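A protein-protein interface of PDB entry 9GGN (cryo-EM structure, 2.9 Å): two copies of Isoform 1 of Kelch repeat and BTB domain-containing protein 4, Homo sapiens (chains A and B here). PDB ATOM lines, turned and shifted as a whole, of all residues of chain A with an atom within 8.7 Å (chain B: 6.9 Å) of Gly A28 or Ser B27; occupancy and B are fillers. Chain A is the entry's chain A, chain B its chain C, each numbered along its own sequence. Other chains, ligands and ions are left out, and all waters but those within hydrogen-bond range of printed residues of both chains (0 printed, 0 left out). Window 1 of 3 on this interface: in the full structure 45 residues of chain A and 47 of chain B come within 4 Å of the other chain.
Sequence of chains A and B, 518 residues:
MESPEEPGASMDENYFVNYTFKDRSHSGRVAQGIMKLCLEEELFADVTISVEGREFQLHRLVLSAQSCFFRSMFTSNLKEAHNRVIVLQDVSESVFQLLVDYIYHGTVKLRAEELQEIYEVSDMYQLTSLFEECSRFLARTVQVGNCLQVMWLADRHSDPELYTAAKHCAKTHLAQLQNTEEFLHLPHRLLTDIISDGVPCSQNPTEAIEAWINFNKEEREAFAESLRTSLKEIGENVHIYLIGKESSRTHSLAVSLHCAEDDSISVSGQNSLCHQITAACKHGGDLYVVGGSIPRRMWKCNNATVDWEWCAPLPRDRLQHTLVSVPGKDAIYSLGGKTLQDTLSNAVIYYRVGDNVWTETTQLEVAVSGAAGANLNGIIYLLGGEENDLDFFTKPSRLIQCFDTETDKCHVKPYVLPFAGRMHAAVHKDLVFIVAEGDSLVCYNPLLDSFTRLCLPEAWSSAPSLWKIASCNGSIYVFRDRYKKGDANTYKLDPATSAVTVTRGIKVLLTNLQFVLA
Ser A27 touches Ala B31. Ala A31 touches Ser B27 (CB to OG, 3.2 Å). Tyr A102 touches Asp B23. CD2 of His B26 touches CA of Gly A106 (3.5 Å). Ser A129 touches Ser B25.
Ser A27 touches its own counterpart, Ser B27. Ser A27 touches Gly B28, and with the chains exchanged Gly A28 touches Ser B27. Ser A27 touches Ala B31, and with the chains exchanged Ala A31 touches Ser B27. Positions printed for both chains: 23, 24, 25, 26, 27, 28, 29, 30, 31 and 32. Of the 8 pairs that touch across the chains among the printed residues, 5 have their exchanged pair printed and touching as well.
Arg A24 touches none of the printed residues of chain B. Gly A28 touches just one residue of chain B: Ser B27 (3.5 Å). Of the printed residues of chain A, Asp B23 touches Tyr A102. Of the printed residues of chain A, His B26 touches Gly A106 (3.5 Å).
The side-chain hydroxyl (OG) of Ser A27 is in hydrogen-bond range of the backbone carbonyl oxygen (O) of Ser B27, at 2.7 Å. The backbone NH (N) of Gly B28 is in hydrogen-bond range of the side-chain hydroxyl (OG) of Ser A27. The backbone NH (N) of Gly A28 sits at hydrogen-bond distance from the side-chain hydroxyl (OG) of Ser B27.
Hydrophobic or aromatic side chains of chain A that line the printed part of chain B: Ala A31 and Tyr A102. Among the printed residues, 8 pairs touch across the chains.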
ATOM      1  N   ASP A  23      17.354   7.175  -2.869  1.00  0.00           N
ATOM      2  CA  ASP A  23      18.180   7.815  -3.886  1.00  0.00           C
ATOM      3  C   ASP A  23      18.030   7.106  -5.221  1.00  0.00           C
ATOM      4  O   ASP A  23      18.081   5.874  -5.285  1.00  0.00           O
ATOM      5  CB  ASP A  23      19.658   7.819  -3.489  1.00  0.00           C
ATOM      6  CG  ASP A  23      19.960   8.791  -2.380  1.00  0.00           C
ATOM      7  OD1 ASP A  23      19.004   9.341  -1.797  1.00  0.00           O
ATOM      8  OD2 ASP A  23      21.157   9.010  -2.103  1.00  0.00           O
ATOM      9  N   ARG A  24      17.845   7.891  -6.283  1.00  0.00           N
ATOM     10  CA  ARG A  24      17.857   7.351  -7.635  1.00  0.00           C
ATOM     11  C   ARG A  24      19.269   7.206  -8.184  1.00  0.00           C
ATOM     12  O   ARG A  24      19.458   6.520  -9.195  1.00  0.00           O
ATOM     13  CB  ARG A  24      17.029   8.239  -8.566  1.00  0.00           C
ATOM     14  N   SER A  25      20.258   7.835  -7.545  1.00  0.00           N
ATOM     15  CA  SER A  25      21.649   7.697  -7.954  1.00  0.00           C
ATOM     16  C   SER A  25      22.247   6.362  -7.533  1.00  0.00           C
ATOM     17  O   SER A  25      23.285   5.963  -8.074  1.00  0.00           O
ATOM     18  CB  SER A  25      22.486   8.839  -7.374  1.00  0.00           C
ATOM     19  OG  SER A  25      22.447   8.830  -5.957  1.00  0.00           O
ATOM     20  N   HIS A  26      21.621   5.675  -6.575  1.00  0.00           N
ATOM     21  CA  HIS A  26      22.151   4.399  -6.105  1.00  0.00           C
ATOM     22  C   HIS A  26      22.164   3.369  -7.226  1.00  0.00           C
ATOM     23  O   HIS A  26      23.133   2.616  -7.375  1.00  0.00           O
ATOM     24  CB  HIS A  26      21.334   3.895  -4.915  1.00  0.00           C
ATOM     25  CG  HIS A  26      21.325   2.404  -4.774  1.00  0.00           C
ATOM     26  ND1 HIS A  26      20.449   1.595  -5.465  1.00  0.00           N
ATOM     27  CD2 HIS A  26      22.088   1.577  -4.022  1.00  0.00           C
ATOM     28  CE1 HIS A  26      20.672   0.333  -5.144  1.00  0.00           C
ATOM     29  NE2 HIS A  26      21.661   0.295  -4.270  1.00  0.00           N
ATOM     30  N   SER A  27      21.091   3.312  -8.018  1.00  0.00           N
ATOM     31  CA  SER A  27      21.060   2.397  -9.153  1.00  0.00           C
ATOM     32  C   SER A  27      22.150   2.742 -10.160  1.00  0.00           C
ATOM     33  O   SER A  27      22.847   1.854 -10.665  1.00  0.00           O
ATOM     34  CB  SER A  27      19.685   2.433  -9.817  1.00  0.00           C
ATOM     35  OG  SER A  27      19.501   1.321 -10.674  1.00  0.00           O
ATOM     36  N   GLY A  28      22.311   4.032 -10.461  1.00  0.00           N
ATOM     37  CA  GLY A  28      23.356   4.438 -11.383  1.00  0.00           C
ATOM     38  C   GLY A  28      24.737   4.034 -10.906  1.00  0.00           C
ATOM     39  O   GLY A  28      25.571   3.588 -11.696  1.00  0.00           O
ATOM     40  N   ARG A  29      24.992   4.165  -9.602  1.00  0.00           N
ATOM     41  CA  ARG A  29      26.309   3.808  -9.083  1.00  0.00           C
ATOM     42  C   ARG A  29      26.514   2.298  -9.077  1.00  0.00           C
ATOM     43  O   ARG A  29      27.578   1.809  -9.474  1.00  0.00           O
ATOM     44  CB  ARG A  29      26.490   4.381  -7.677  1.00  0.00           C
ATOM     45  N   VAL A  30      25.508   1.540  -8.629  1.00  0.00           N
ATOM     46  CA  VAL A  30      25.609   0.085  -8.604  1.00  0.00           C
ATOM     47  C   VAL A  30      25.554  -0.504 -10.008  1.00  0.00           C
ATOM     48  O   VAL A  30      25.775  -1.707 -10.190  1.00  0.00           O
ATOM     49  CB  VAL A  30      24.504  -0.463  -7.671  1.00  0.00           C
ATOM     50  CG1 VAL A  30      24.490  -1.987  -7.619  1.00  0.00           C
ATOM     51  CG2 VAL A  30      24.681   0.100  -6.269  1.00  0.00           C
ATOM     52  N   ALA A  31      25.316   0.327 -11.021  1.00  0.00           N
ATOM     53  CA  ALA A  31      25.520  -0.104 -12.398  1.00  0.00           C
ATOM     54  C   ALA A  31      26.910   0.271 -12.908  1.00  0.00           C
ATOM     55  O   ALA A  31      27.604  -0.563 -13.499  1.00  0.00           O
ATOM     56  CB  ALA A  31      24.444   0.496 -13.305  1.00  0.00           C
ATOM     57  N   GLN A  32      27.328   1.519 -12.682  1.00  0.00           N
ATOM     58  CA  GLN A  32      28.581   1.997 -13.255  1.00  0.00           C
ATOM     59  C   GLN A  32      29.785   1.329 -12.605  1.00  0.00           C
ATOM     60  O   GLN A  32      30.728   0.931 -13.301  1.00  0.00           O
ATOM     61  CB  GLN A  32      28.674   3.517 -13.116  1.00  0.00           C
ATOM     62  N   GLY A  33      29.785   1.203 -11.275  1.00  0.00           N
ATOM     63  CA  GLY A  33      30.875   0.501 -10.616  1.00  0.00           C
ATOM     64  C   GLY A  33      30.961  -0.957 -11.018  1.00  0.00           C
ATOM     65  O   GLY A  33      32.057  -1.502 -11.181  1.00  0.00           O
ATOM     66  N   ILE A  34      29.810  -1.614 -11.172  1.00  0.00           N
ATOM     67  CA  ILE A  34      29.799  -2.994 -11.650  1.00  0.00           C
ATOM     68  C   ILE A  34      30.403  -3.076 -13.047  1.00  0.00           C
ATOM     69  O   ILE A  34      31.259  -3.922 -13.322  1.00  0.00           O
ATOM     70  CB  ILE A  34      28.373  -3.579 -11.609  1.00  0.00           C
ATOM     71  CG1 ILE A  34      28.025  -4.127 -10.217  1.00  0.00           C
ATOM     72  CG2 ILE A  34      28.206  -4.671 -12.657  1.00  0.00           C
ATOM     73  CD1 ILE A  34      28.232  -3.182  -9.054  1.00  0.00           C
ATOM     74  N   MET A  35      29.987  -2.180 -13.943  1.00  0.00           N
ATOM     75  CA  MET A  35      30.523  -2.198 -15.301  1.00  0.00           C
ATOM     76  C   MET A  35      32.028  -1.966 -15.307  1.00  0.00           C
ATOM     77  O   MET A  35      32.763  -2.616 -16.060  1.00  0.00           O
ATOM     78  CB  MET A  35      29.813  -1.151 -16.159  1.00  0.00           C
ATOM     79  N   TYR A 102      26.450  -7.520 -22.688  1.00  0.00           N
ATOM     80  CA  TYR A 102      25.157  -7.008 -22.250  1.00  0.00           C
ATOM     81  C   TYR A 102      25.043  -7.074 -20.732  1.00  0.00           C
ATOM     82  O   TYR A 102      24.917  -6.047 -20.057  1.00  0.00           O
ATOM     83  CB  TYR A 102      24.024  -7.804 -22.902  1.00  0.00           C
ATOM     84  CG  TYR A 102      22.648  -7.199 -22.711  1.00  0.00           C
ATOM     85  CD1 TYR A 102      22.491  -5.918 -22.194  1.00  0.00           C
ATOM     86  CD2 TYR A 102      21.505  -7.915 -23.035  1.00  0.00           C
ATOM     87  CE1 TYR A 102      21.241  -5.367 -22.015  1.00  0.00           C
ATOM     88  CE2 TYR A 102      20.250  -7.371 -22.855  1.00  0.00           C
ATOM     89  CZ  TYR A 102      20.122  -6.098 -22.348  1.00  0.00           C
ATOM     90  OH  TYR A 102      18.873  -5.553 -22.171  1.00  0.00           O
ATOM     91  N   HIS A 105      27.575  -4.569 -19.080  1.00  0.00           N
ATOM     92  CA  HIS A 105      27.596  -3.150 -19.403  1.00  0.00           C
ATOM     93  C   HIS A 105      26.269  -2.613 -19.919  1.00  0.00           C
ATOM     94  O   HIS A 105      26.129  -1.392 -20.055  1.00  0.00           O
ATOM     95  CB  HIS A 105      28.688  -2.853 -20.443  1.00  0.00           C
ATOM     96  N   GLY A 106      25.295  -3.477 -20.206  1.00  0.00           N
ATOM     97  CA  GLY A 106      24.006  -3.060 -20.718  1.00  0.00           C
ATOM     98  C   GLY A 106      23.983  -2.532 -22.136  1.00  0.00           C
ATOM     99  O   GLY A 106      22.891  -2.367 -22.692  1.00  0.00           O
ATOM    100  N   SER A 129      14.445  -8.050 -21.524  1.00  0.00           N
ATOM    101  CA  SER A 129      14.738  -6.872 -22.337  1.00  0.00           C
ATOM    102  C   SER A 129      15.322  -7.272 -23.686  1.00  0.00           C
ATOM    103  O   SER A 129      14.878  -6.794 -24.739  1.00  0.00           O
ATOM    104  CB  SER A 129      15.692  -5.945 -21.586  1.00  0.00           C
ATOM    105  OG  SER A 129      15.049  -5.343 -20.477  1.00  0.00           O
ATOM    106  N   ASP B  23      20.110   0.839 -22.828  1.00  0.00           N
ATOM    107  CA  ASP B  23      18.888   0.755 -22.038  1.00  0.00           C
ATOM    108  C   ASP B  23      19.079   1.415 -20.683  1.00  0.00           C
ATOM    109  O   ASP B  23      20.086   1.182 -20.010  1.00  0.00           O
ATOM    110  CB  ASP B  23      18.456  -0.698 -21.825  1.00  0.00           C
ATOM    111  CG  ASP B  23      17.901  -1.329 -23.074  1.00  0.00           C
ATOM    112  OD1 ASP B  23      18.005  -0.705 -24.149  1.00  0.00           O
ATOM    113  OD2 ASP B  23      17.350  -2.445 -22.973  1.00  0.00           O
ATOM    114  N   ARG B  24      18.105   2.237 -20.289  1.00  0.00           N
ATOM    115  CA  ARG B  24      18.085   2.796 -18.946  1.00  0.00           C
ATOM    116  C   ARG B  24      17.471   1.839 -17.934  1.00  0.00           C
ATOM    117  O   ARG B  24      17.627   2.052 -16.727  1.00  0.00           O
ATOM    118  CB  ARG B  24      17.316   4.120 -18.935  1.00  0.00           C
ATOM    119  N   SER B  25      16.780   0.795 -18.398  1.00  0.00           N
ATOM    120  CA  SER B  25      16.219  -0.214 -17.509  1.00  0.00           C
ATOM    121  C   SER B  25      17.277  -1.171 -16.979  1.00  0.00           C
ATOM    122  O   SER B  25      17.029  -1.861 -15.984  1.00  0.00           O
ATOM    123  CB  SER B  25      15.127  -1.005 -18.230  1.00  0.00           C
ATOM    124  OG  SER B  25      15.647  -1.670 -19.368  1.00  0.00           O
ATOM    125  N   HIS B  26      18.442  -1.233 -17.631  1.00  0.00           N
ATOM    126  CA  HIS B  26      19.492  -2.145 -17.192  1.00  0.00           C
ATOM    127  C   HIS B  26      19.974  -1.789 -15.792  1.00  0.00           C
ATOM    128  O   HIS B  26      20.191  -2.676 -14.960  1.00  0.00           O
ATOM    129  CB  HIS B  26      20.652  -2.127 -18.187  1.00  0.00           C
ATOM    130  CG  HIS B  26      21.980  -2.455 -17.576  1.00  0.00           C
ATOM    131  ND1 HIS B  26      22.763  -1.513 -16.944  1.00  0.00           N
ATOM    132  CD2 HIS B  26      22.661  -3.622 -17.500  1.00  0.00           C
ATOM    133  CE1 HIS B  26      23.870  -2.087 -16.506  1.00  0.00           C
ATOM    134  NE2 HIS B  26      23.833  -3.366 -16.831  1.00  0.00           N
ATOM    135  N   SER B  27      20.156  -0.495 -15.519  1.00  0.00           N
ATOM    136  CA  SER B  27      20.551  -0.074 -14.179  1.00  0.00           C
ATOM    137  C   SER B  27      19.484  -0.442 -13.157  1.00  0.00           C
ATOM    138  O   SER B  27      19.797  -0.946 -12.070  1.00  0.00           O
ATOM    139  CB  SER B  27      20.815   1.431 -14.161  1.00  0.00           C
ATOM    140  OG  SER B  27      21.533   1.809 -13.001  1.00  0.00           O
ATOM    141  N   GLY B  28      18.214  -0.200 -13.491  1.00  0.00           N
ATOM    142  CA  GLY B  28      17.142  -0.561 -12.579  1.00  0.00           C
ATOM    143  C   GLY B  28      17.125  -2.044 -12.267  1.00  0.00           C
ATOM    144  O   GLY B  28      16.907  -2.444 -11.122  1.00  0.00           O
ATOM    145  N   ARG B  29      17.373  -2.882 -13.276  1.00  0.00           N
ATOM    146  CA  ARG B  29      17.353  -4.322 -13.044  1.00  0.00           C
ATOM    147  C   ARG B  29      18.566  -4.771 -12.236  1.00  0.00           C
ATOM    148  O   ARG B  29      18.435  -5.568 -11.301  1.00  0.00           O
ATOM    149  CB  ARG B  29      17.287  -5.067 -14.377  1.00  0.00           C
ATOM    150  N   VAL B  30      19.757  -4.273 -12.584  1.00  0.00           N
ATOM    151  CA  VAL B  30      20.970  -4.633 -11.857  1.00  0.00           C
ATOM    152  C   VAL B  30      21.003  -3.997 -10.473  1.00  0.00           C
ATOM    153  O   VAL B  30      21.881  -4.310  -9.662  1.00  0.00           O
ATOM    154  CB  VAL B  30      22.189  -4.254 -12.730  1.00  0.00           C
ATOM    155  CG1 VAL B  30      23.514  -4.540 -12.033  1.00  0.00           C
ATOM    156  CG2 VAL B  30      22.130  -4.997 -14.056  1.00  0.00           C
ATOM    157  N   ALA B  31      20.029  -3.145 -10.159  1.00  0.00           N
ATOM    158  CA  ALA B  31      19.836  -2.714  -8.780  1.00  0.00           C
ATOM    159  C   ALA B  31      18.804  -3.576  -8.058  1.00  0.00           C
ATOM    160  O   ALA B  31      19.043  -4.024  -6.931  1.00  0.00           O
ATOM    161  CB  ALA B  31      19.419  -1.243  -8.740  1.00  0.00           C
ATOM    162  N   GLN B  32      17.655  -3.818  -8.694  1.00  0.00           N
ATOM    163  CA  GLN B  32      16.565  -4.515  -8.021  1.00  0.00           C
ATOM    164  C   GLN B  32      16.901  -5.980  -7.778  1.00  0.00           C
ATOM    165  O   GLN B  32      16.636  -6.508  -6.691  1.00  0.00           O
ATOM    166  CB  GLN B  32      15.279  -4.389  -8.837  1.00  0.00           C
